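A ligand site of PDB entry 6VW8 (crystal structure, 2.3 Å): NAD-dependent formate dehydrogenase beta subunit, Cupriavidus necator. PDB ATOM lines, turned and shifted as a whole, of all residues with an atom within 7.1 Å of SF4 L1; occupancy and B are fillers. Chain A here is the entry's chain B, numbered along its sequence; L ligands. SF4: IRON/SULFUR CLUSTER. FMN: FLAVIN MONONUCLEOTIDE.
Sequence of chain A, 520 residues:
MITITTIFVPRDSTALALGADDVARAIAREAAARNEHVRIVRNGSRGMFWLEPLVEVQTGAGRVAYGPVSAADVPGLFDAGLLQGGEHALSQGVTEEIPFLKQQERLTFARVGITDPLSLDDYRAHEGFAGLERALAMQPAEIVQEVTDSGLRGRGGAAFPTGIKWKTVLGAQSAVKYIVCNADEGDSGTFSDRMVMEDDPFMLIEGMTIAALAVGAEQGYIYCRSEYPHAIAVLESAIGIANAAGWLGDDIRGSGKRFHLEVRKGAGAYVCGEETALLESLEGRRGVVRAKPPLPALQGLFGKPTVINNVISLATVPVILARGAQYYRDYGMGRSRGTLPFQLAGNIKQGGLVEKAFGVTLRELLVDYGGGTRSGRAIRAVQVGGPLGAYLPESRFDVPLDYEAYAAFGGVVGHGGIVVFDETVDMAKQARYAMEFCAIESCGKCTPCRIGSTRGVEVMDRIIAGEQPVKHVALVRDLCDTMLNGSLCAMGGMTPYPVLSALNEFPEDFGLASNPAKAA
OG of Ser 442 sits close to SG of Cys 449 (3.3 Å).
The side-chain sulfur of Cys 443 lies close to the backbone NH of Val 289, 3.5 Å away.
SG of Cys 489 lies close to N of Met 491 (3.4 Å).
O of Val 289 is in hydrogen-bond range of NZ of Lys 445 (2.7 Å).
O of Gly 492 lies close to OG of Ser 487 (3.5 Å).
The side-chain hydroxyl (OG) of Ser 442 lies close to the backbone NH (N) of Gly 444 (3.0 Å).
OG of Ser 442 lies close to N of Arg 450, 3.4 Å away.
The backbone carbonyl oxygen (O) of Gly 444 lies within hydrogen-bond range of the guanidinium group (NE) of Arg 450, 3.2 Å away.
Residues that only touch SF4 L1: Val 271 (3.7 Å), Val 289 (3.5 Å), Ser 487 (3.6 Å) and Met 491 (3.6 Å).
Hydrophobic or aromatic side chains within 4 Å of SF4 L1: Val 271, Val 289, Leu 488 and Met 491.
13 residues have an atom within 4 Å of SF4 L1: Val 271, Val 289, Ser 442, Cys 443, Gly 444, Lys 445, Cys 446, Cys 449, Ser 487, Leu 488, Cys 489, Met 491 and Gly 492.
The nearest printed residue that does not touch SF4 L1 is Gly 493 (4.7 Å).
The backbone NH (N) of Cys 446 sits close to a sulfur (S3) of SF4 L1 (3.1 Å).
An iron atom (FE4) of SF4 L1 is bound by the side-chain sulfur (SG) of Cys 446 (2.4 Å).
SG of Cys 449 binds FE2 of SF4 L1, at 2.4 Å.
N of Cys 443 sits close to S4 of SF4 L1 (3.6 Å).
The side-chain sulfur (SG) of Cys 443 binds an iron atom (FE1) of SF4 L1 (2.4 Å).
N of Cys 489 sits close to S1 of SF4 L1 (3.7 Å).
SG of Cys 489 is bound to FE3 of SF4 L1 (2.5 Å).
The backbone NH (N) of Lys 445 lies close to a sulfur (S3) of SF4 L1, at 3.3 Å.
A sulfur (S1) of SF4 L1 sits close to the backbone NH (N) of Gly 492, 3.3 Å away.
The side-chain hydroxyl (OG) of Ser 442 lies close to a sulfur (S3) of SF4 L1, 3.6 Å away.
The backbone NH (N) of Gly 444 sits close to a sulfur (S3) of SF4 L1 (3.6 Å).
A sulfur (S1) of SF4 L1 sits close to the backbone NH (N) of Leu 488 (3.7 Å).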
ATOM      1  N   VAL A 271      15.437  -4.551 -18.920  1.00  0.00           N
ATOM      2  CA  VAL A 271      14.875  -3.882 -17.748  1.00  0.00           C
ATOM      3  C   VAL A 271      15.180  -4.621 -16.446  1.00  0.00           C
ATOM      4  O   VAL A 271      15.023  -4.030 -15.356  1.00  0.00           O
ATOM      5  CB  VAL A 271      13.364  -3.649 -17.967  1.00  0.00           C
ATOM      6  CG1 VAL A 271      12.635  -3.098 -16.705  1.00  0.00           C
ATOM      7  CG2 VAL A 271      13.212  -2.650 -19.070  1.00  0.00           C
ATOM      8  N   GLU A 274      17.297  -2.963 -13.954  1.00  0.00           N
ATOM      9  CA  GLU A 274      16.704  -2.070 -12.971  1.00  0.00           C
ATOM     10  C   GLU A 274      16.584  -2.798 -11.650  1.00  0.00           C
ATOM     11  O   GLU A 274      16.049  -3.895 -11.596  1.00  0.00           O
ATOM     12  CB  GLU A 274      15.325  -1.591 -13.437  1.00  0.00           C
ATOM     13  CG  GLU A 274      14.825  -0.347 -12.723  1.00  0.00           C
ATOM     14  CD  GLU A 274      14.200  -0.623 -11.378  1.00  0.00           C
ATOM     15  OE1 GLU A 274      13.658  -1.731 -11.152  1.00  0.00           O
ATOM     16  OE2 GLU A 274      14.242   0.287 -10.529  1.00  0.00           O
ATOM     17  N   GLY A 287      10.063  -9.566 -14.756  1.00  0.00           N
ATOM     18  CA  GLY A 287      10.884  -8.451 -14.329  1.00  0.00           C
ATOM     19  C   GLY A 287      10.196  -7.090 -14.409  1.00  0.00           C
ATOM     20  O   GLY A 287      10.624  -6.223 -15.157  1.00  0.00           O
ATOM     21  N   VAL A 288       9.112  -6.930 -13.640  1.00  0.00           N
ATOM     22  CA  VAL A 288       8.348  -5.688 -13.613  1.00  0.00           C
ATOM     23  C   VAL A 288       8.874  -4.807 -12.472  1.00  0.00           C
ATOM     24  O   VAL A 288       9.021  -5.262 -11.331  1.00  0.00           O
ATOM     25  CB  VAL A 288       6.857  -5.980 -13.456  1.00  0.00           C
ATOM     26  CG1 VAL A 288       6.068  -4.680 -13.366  1.00  0.00           C
ATOM     27  CG2 VAL A 288       6.378  -6.882 -14.627  1.00  0.00           C
ATOM     28  N   VAL A 289       9.193  -3.553 -12.785  1.00  0.00           N
ATOM     29  CA  VAL A 289       9.710  -2.629 -11.747  1.00  0.00           C
ATOM     30  C   VAL A 289       8.730  -2.533 -10.565  1.00  0.00           C
ATOM     31  O   VAL A 289       7.562  -2.435 -10.774  1.00  0.00           O
ATOM     32  CB  VAL A 289      10.070  -1.266 -12.360  1.00  0.00           C
ATOM     33  CG1 VAL A 289      10.583  -0.311 -11.316  1.00  0.00           C
ATOM     34  CG2 VAL A 289      11.019  -1.356 -13.531  1.00  0.00           C
ATOM     35  N   ARG A 290       9.231  -2.618  -9.342  1.00  0.00           N
ATOM     36  CA  ARG A 290       8.372  -2.502  -8.165  1.00  0.00           C
ATOM     37  C   ARG A 290       8.181  -1.023  -7.867  1.00  0.00           C
ATOM     38  O   ARG A 290       9.021  -0.262  -8.170  1.00  0.00           O
ATOM     39  CB  ARG A 290       8.966  -3.113  -6.897  1.00  0.00           C
ATOM     40  CG  ARG A 290       9.439  -4.547  -7.004  1.00  0.00           C
ATOM     41  CD  ARG A 290      10.111  -5.011  -5.722  1.00  0.00           C
ATOM     42  NE  ARG A 290      10.180  -6.440  -5.628  1.00  0.00           N
ATOM     43  CZ  ARG A 290      10.759  -7.134  -4.676  1.00  0.00           C
ATOM     44  NH1 ARG A 290      11.349  -6.536  -3.669  1.00  0.00           N
ATOM     45  NH2 ARG A 290      10.744  -8.449  -4.727  1.00  0.00           N
ATOM     46  N   LYS A 292       7.992   2.139  -5.276  1.00  0.00           N
ATOM     47  CA  LYS A 292       8.809   2.379  -4.078  1.00  0.00           C
ATOM     48  C   LYS A 292       8.111   3.104  -2.915  1.00  0.00           C
ATOM     49  O   LYS A 292       8.230   4.299  -2.814  1.00  0.00           O
ATOM     50  CB  LYS A 292      10.137   3.040  -4.452  1.00  0.00           C
ATOM     51  CG  LYS A 292      10.961   2.213  -5.411  1.00  0.00           C
ATOM     52  CD  LYS A 292      10.549   2.315  -6.846  1.00  0.00           C
ATOM     53  CE  LYS A 292      11.578   1.642  -7.728  1.00  0.00           C
ATOM     54  NZ  LYS A 292      11.420   2.011  -9.137  1.00  0.00           N
ATOM     55  N   CYS A 438      13.066   0.830 -26.771  1.00  0.00           N
ATOM     56  CA  CYS A 438      12.177   0.961 -25.619  1.00  0.00           C
ATOM     57  C   CYS A 438      10.975   0.026 -25.750  1.00  0.00           C
ATOM     58  O   CYS A 438      10.598  -0.651 -24.785  1.00  0.00           O
ATOM     59  CB  CYS A 438      11.715   2.415 -25.442  1.00  0.00           C
ATOM     60  SG  CYS A 438      10.859   2.727 -23.839  1.00  0.00           S
ATOM     61  N   GLU A 441      12.031  -3.569 -24.840  1.00  0.00           N
ATOM     62  CA  GLU A 441      12.410  -3.928 -23.472  1.00  0.00           C
ATOM     63  C   GLU A 441      11.430  -3.494 -22.395  1.00  0.00           C
ATOM     64  O   GLU A 441      11.596  -3.910 -21.245  1.00  0.00           O
ATOM     65  CB  GLU A 441      13.778  -3.328 -23.147  1.00  0.00           C
ATOM     66  CG  GLU A 441      14.817  -3.637 -24.167  1.00  0.00           C
ATOM     67  CD  GLU A 441      15.214  -5.098 -24.129  1.00  0.00           C
ATOM     68  OE1 GLU A 441      14.885  -5.813 -23.138  1.00  0.00           O
ATOM     69  OE2 GLU A 441      15.858  -5.539 -25.098  1.00  0.00           O
ATOM     70  N   SER A 442      10.427  -2.664 -22.726  1.00  0.00           N
ATOM     71  CA  SER A 442       9.498  -2.126 -21.722  1.00  0.00           C
ATOM     72  C   SER A 442       8.961  -3.258 -20.844  1.00  0.00           C
ATOM     73  O   SER A 442       8.443  -4.257 -21.348  1.00  0.00           O
ATOM     74  CB  SER A 442       8.333  -1.387 -22.404  1.00  0.00           C
ATOM     75  OG  SER A 442       7.236  -1.124 -21.530  1.00  0.00           O
ATOM     76  N   CYS A 443       9.138  -3.141 -19.526  1.00  0.00           N
ATOM     77  CA  CYS A 443       8.474  -4.113 -18.660  1.00  0.00           C
ATOM     78  C   CYS A 443       6.955  -4.111 -18.827  1.00  0.00           C
ATOM     79  O   CYS A 443       6.312  -5.116 -18.528  1.00  0.00           O
ATOM     80  CB  CYS A 443       8.981  -3.981 -17.227  1.00  0.00           C
ATOM     81  SG  CYS A 443       8.136  -2.934 -16.105  1.00  0.00           S
ATOM     82  N   GLY A 444       6.368  -3.029 -19.331  1.00  0.00           N
ATOM     83  CA  GLY A 444       4.943  -3.014 -19.596  1.00  0.00           C
ATOM     84  C   GLY A 444       4.070  -2.293 -18.582  1.00  0.00           C
ATOM     85  O   GLY A 444       2.854  -2.239 -18.769  1.00  0.00           O
ATOM     86  N   LYS A 445       4.648  -1.776 -17.505  1.00  0.00           N
ATOM     87  CA  LYS A 445       3.850  -1.172 -16.447  1.00  0.00           C
ATOM     88  C   LYS A 445       3.295   0.205 -16.850  1.00  0.00           C
ATOM     89  O   LYS A 445       2.250   0.604 -16.349  1.00  0.00           O
ATOM     90  CB  LYS A 445       4.701  -1.068 -15.187  1.00  0.00           C
ATOM     91  CG  LYS A 445       3.956  -1.045 -13.886  1.00  0.00           C
ATOM     92  CD  LYS A 445       4.933  -0.718 -12.763  1.00  0.00           C
ATOM     93  CE  LYS A 445       4.531  -1.443 -11.486  1.00  0.00           C
ATOM     94  NZ  LYS A 445       5.332  -0.971 -10.322  1.00  0.00           N
ATOM     95  N   CYS A 446       3.965   0.925 -17.752  1.00  0.00           N
ATOM     96  CA  CYS A 446       3.672   2.334 -18.025  1.00  0.00           C
ATOM     97  C   CYS A 446       3.272   2.536 -19.479  1.00  0.00           C
ATOM     98  O   CYS A 446       3.948   2.051 -20.387  1.00  0.00           O
ATOM     99  CB  CYS A 446       4.885   3.218 -17.689  1.00  0.00           C
ATOM    100  SG  CYS A 446       5.551   2.992 -16.018  1.00  0.00           S
ATOM    101  N   THR A 447       2.205   3.310 -19.717  1.00  0.00           N
ATOM    102  CA  THR A 447       1.696   3.392 -21.083  1.00  0.00           C
ATOM    103  C   THR A 447       2.630   4.096 -22.043  1.00  0.00           C
ATOM    104  O   THR A 447       2.881   3.546 -23.135  1.00  0.00           O
ATOM    105  CB  THR A 447       0.305   4.014 -21.087  1.00  0.00           C
ATOM    106  OG1 THR A 447      -0.532   3.220 -20.244  1.00  0.00           O
ATOM    107  CG2 THR A 447      -0.249   4.041 -22.494  1.00  0.00           C
ATOM    108  N   PRO A 448       3.174   5.281 -21.748  1.00  0.00           N
ATOM    109  CA  PRO A 448       4.140   5.867 -22.702  1.00  0.00           C
ATOM    110  C   PRO A 448       5.325   4.944 -22.989  1.00  0.00           C
ATOM    111  O   PRO A 448       5.806   4.883 -24.129  1.00  0.00           O
ATOM    112  CB  PRO A 448       4.560   7.160 -21.994  1.00  0.00           C
ATOM    113  CG  PRO A 448       3.449   7.462 -21.021  1.00  0.00           C
ATOM    114  CD  PRO A 448       3.014   6.123 -20.556  1.00  0.00           C
ATOM    115  N   CYS A 449       5.773   4.166 -21.993  1.00  0.00           N
ATOM    116  CA  CYS A 449       6.898   3.265 -22.253  1.00  0.00           C
ATOM    117  C   CYS A 449       6.480   2.061 -23.087  1.00  0.00           C
ATOM    118  O   CYS A 449       7.170   1.693 -24.047  1.00  0.00           O
ATOM    119  CB  CYS A 449       7.501   2.785 -20.933  1.00  0.00           C
ATOM    120  SG  CYS A 449       8.902   1.704 -21.176  1.00  0.00           S
ATOM    121  N   ARG A 450       5.340   1.455 -22.772  1.00  0.00           N
ATOM    122  CA  ARG A 450       4.966   0.235 -23.471  1.00  0.00           C
ATOM    123  C   ARG A 450       4.493   0.542 -24.883  1.00  0.00           C
ATOM    124  O   ARG A 450       4.931  -0.095 -25.845  1.00  0.00           O
ATOM    125  CB  ARG A 450       3.899  -0.527 -22.691  1.00  0.00           C
ATOM    126  CG  ARG A 450       3.567  -1.900 -23.317  1.00  0.00           C
ATOM    127  CD  ARG A 450       2.439  -2.640 -22.617  1.00  0.00           C
ATOM    128  NE  ARG A 450       1.698  -1.754 -21.735  1.00  0.00           N
ATOM    129  CZ  ARG A 450       0.417  -1.471 -21.857  1.00  0.00           C
ATOM    130  NH1 ARG A 450      -0.313  -2.026 -22.823  1.00  0.00           N
ATOM    131  NH2 ARG A 450      -0.132  -0.624 -20.983  1.00  0.00           N
ATOM    132  N   MET A 483       6.895  10.806 -21.995  1.00  0.00           N
ATOM    133  CA  MET A 483       7.713   9.756 -21.378  1.00  0.00           C
ATOM    134  C   MET A 483       8.503  10.283 -20.188  1.00  0.00           C
ATOM    135  O   MET A 483       8.669   9.573 -19.188  1.00  0.00           O
ATOM    136  CB  MET A 483       8.660   9.148 -22.421  1.00  0.00           C
ATOM    137  CG  MET A 483       7.946   8.395 -23.508  1.00  0.00           C
ATOM    138  SD  MET A 483       9.064   7.826 -24.794  1.00  0.00           S
ATOM    139  CE  MET A 483       9.405   6.124 -24.224  1.00  0.00           C
ATOM    140  N   GLY A 486       5.800  10.428 -17.205  1.00  0.00           N
ATOM    141  CA  GLY A 486       4.970   9.302 -16.830  1.00  0.00           C
ATOM    142  C   GLY A 486       5.644   7.941 -16.902  1.00  0.00           C
ATOM    143  O   GLY A 486       5.005   6.934 -17.206  1.00  0.00           O
ATOM    144  N   SER A 487       6.938   7.887 -16.594  1.00  0.00           N
ATOM    145  CA  SER A 487       7.661   6.625 -16.578  1.00  0.00           C
ATOM    146  C   SER A 487       8.054   6.282 -15.156  1.00  0.00           C
ATOM    147  O   SER A 487       8.504   7.148 -14.412  1.00  0.00           O
ATOM    148  CB  SER A 487       8.916   6.681 -17.451  1.00  0.00           C
ATOM    149  OG  SER A 487       8.586   6.780 -18.824  1.00  0.00           O
ATOM    150  N   LEU A 488       7.872   5.026 -14.766  1.00  0.00           N
ATOM    151  CA  LEU A 488       8.209   4.665 -13.410  1.00  0.00           C
ATOM    152  C   LEU A 488       9.701   4.383 -13.245  1.00  0.00           C
ATOM    153  O   LEU A 488      10.158   4.194 -12.103  1.00  0.00           O
ATOM    154  CB  LEU A 488       7.381   3.456 -12.963  1.00  0.00           C
ATOM    155  N   CYS A 489      10.460   4.341 -14.339  1.00  0.00           N
ATOM    156  CA  CYS A 489      11.903   4.108 -14.221  1.00  0.00           C
ATOM    157  C   CYS A 489      12.601   4.699 -15.442  1.00  0.00           C
ATOM    158  O   CYS A 489      11.972   5.040 -16.448  1.00  0.00           O
ATOM    159  CB  CYS A 489      12.205   2.607 -14.033  1.00  0.00           C
ATOM    160  SG  CYS A 489      12.488   1.615 -15.512  1.00  0.00           S
ATOM    161  N   ALA A 490      13.929   4.771 -15.356  1.00  0.00           N
ATOM    162  CA  ALA A 490      14.685   5.437 -16.401  1.00  0.00           C
ATOM    163  C   ALA A 490      14.597   4.751 -17.762  1.00  0.00           C
ATOM    164  O   ALA A 490      15.025   5.349 -18.753  1.00  0.00           O
ATOM    165  CB  ALA A 490      16.151   5.564 -15.979  1.00  0.00           C
ATOM    166  N   MET A 491      14.061   3.543 -17.863  1.00  0.00           N
ATOM    167  CA  MET A 491      13.877   2.973 -19.200  1.00  0.00           C
ATOM    168  C   MET A 491      12.916   3.827 -20.013  1.00  0.00           C
ATOM    169  O   MET A 491      13.226   4.273 -21.114  1.00  0.00           O
ATOM    170  CB  MET A 491      13.379   1.534 -19.121  1.00  0.00           C
ATOM    171  CG  MET A 491      12.833   1.006 -20.439  1.00  0.00           C
ATOM    172  SD  MET A 491      14.165   0.302 -21.400  1.00  0.00           S
ATOM    173  CE  MET A 491      14.670   1.678 -22.440  1.00  0.00           C
ATOM    174  N   GLY A 492      11.730   4.077 -19.472  1.00  0.00           N
ATOM    175  CA  GLY A 492      10.842   5.001 -20.123  1.00  0.00           C
ATOM    176  C   GLY A 492      11.306   6.433 -19.969  1.00  0.00           C
ATOM    177  O   GLY A 492      11.297   7.208 -20.935  1.00  0.00           O
ATOM    178  N   GLY A 493      11.752   6.814 -18.770  1.00  0.00           N
ATOM    179  CA  GLY A 493      11.993   8.221 -18.503  1.00  0.00           C
ATOM    180  C   GLY A 493      13.221   8.777 -19.187  1.00  0.00           C
ATOM    181  O   GLY A 493      13.311  10.002 -19.357  1.00  0.00           O
HETATM  182 FE1  SF4 L   1       8.490  -0.663 -16.944  1.00  0.00          FE
HETATM  183 FE2  SF4 L   1       9.059   1.218 -18.830  1.00  0.00          FE
HETATM  184 FE3  SF4 L   1      10.201   1.361 -16.373  1.00  0.00          FE
HETATM  185 FE4  SF4 L   1       7.496   1.842 -16.699  1.00  0.00          FE
HETATM  186  S1  SF4 L   1       9.215   3.082 -17.570  1.00  0.00           S
HETATM  187  S2  SF4 L   1       8.503   0.548 -15.068  1.00  0.00           S
HETATM  188  S3  SF4 L   1       6.985   0.394 -18.312  1.00  0.00           S
HETATM  189  S4  SF4 L   1      10.549  -0.234 -17.871  1.00  0.00           S
HETATM  190  N1  FMN L   2      22.693  -1.116 -12.843  1.00  0.00           N
HETATM  191  C2  FMN L   2      23.787  -2.065 -13.095  1.00  0.00           C
HETATM  192  O2  FMN L   2      24.671  -2.177 -12.311  1.00  0.00           O
HETATM  193  N3  FMN L   2      23.813  -2.870 -14.347  1.00  0.00           N
HETATM  194  C4  FMN L   2      22.738  -2.721 -15.312  1.00  0.00           C
HETATM  195  O4  FMN L   2      22.702  -3.353 -16.305  1.00  0.00           O
HETATM  196  C4A FMN L   2      21.616  -1.758 -15.020  1.00  0.00           C
HETATM  197  N5  FMN L   2      20.546  -1.622 -15.983  1.00  0.00           N
HETATM  198  C5A FMN L   2      19.421  -0.684 -15.729  1.00  0.00           C
HETATM  199  C6  FMN L   2      18.397  -0.613 -16.680  1.00  0.00           C
HETATM  200  C7  FMN L   2      17.325   0.271 -16.479  1.00  0.00           C
HETATM  201  C7M FMN L   2      16.359   0.154 -17.681  1.00  0.00           C
HETATM  202  C8  FMN L   2      17.260   1.080 -15.318  1.00  0.00           C
HETATM  203  C8M FMN L   2      16.127   2.098 -15.001  1.00  0.00           C
HETATM  204  C9  FMN L   2      18.316   0.983 -14.364  1.00  0.00           C
HETATM  205  C9A FMN L   2      19.401   0.097 -14.562  1.00  0.00           C
HETATM  206  N10 FMN L   2      20.531  -0.052 -13.580  1.00  0.00           N
HETATM  207  C10 FMN L   2      21.622  -0.970 -13.826  1.00  0.00           C
HETATM  208  C1' FMN L   2      20.623   0.721 -12.321  1.00  0.00           C
HETATM  209  C2' FMN L   2      20.138  -0.083 -11.124  1.00  0.00           C
HETATM  210  O2' FMN L   2      18.768   0.110 -11.128  1.00  0.00           O
HETATM  211  C3' FMN L   2      20.789   0.513  -9.881  1.00  0.00           C
HETATM  212  O3' FMN L   2      20.891   1.902 -10.021  1.00  0.00           O
HETATM  213  C4' FMN L   2      22.216  -0.017  -9.689  1.00  0.00           C
HETATM  214  O4' FMN L   2      22.325  -1.383 -10.001  1.00  0.00           O
HETATM  215  C5' FMN L   2      22.572   0.220  -8.228  1.00  0.00           C
HETATM  216  O5' FMN L   2      23.889  -0.283  -8.012  1.00  0.00           O
HETATM  217  P   FMN L   2      25.039   0.879  -7.772  1.00  0.00           P
HETATM  218  O1P FMN L   2      26.364   0.253  -7.364  1.00  0.00           O
HETATM  219  O2P FMN L   2      24.518   1.806  -6.687  1.00  0.00           O
HETATM  220  O3P FMN L   2      25.177   1.638  -9.089  1.00  0.00           O
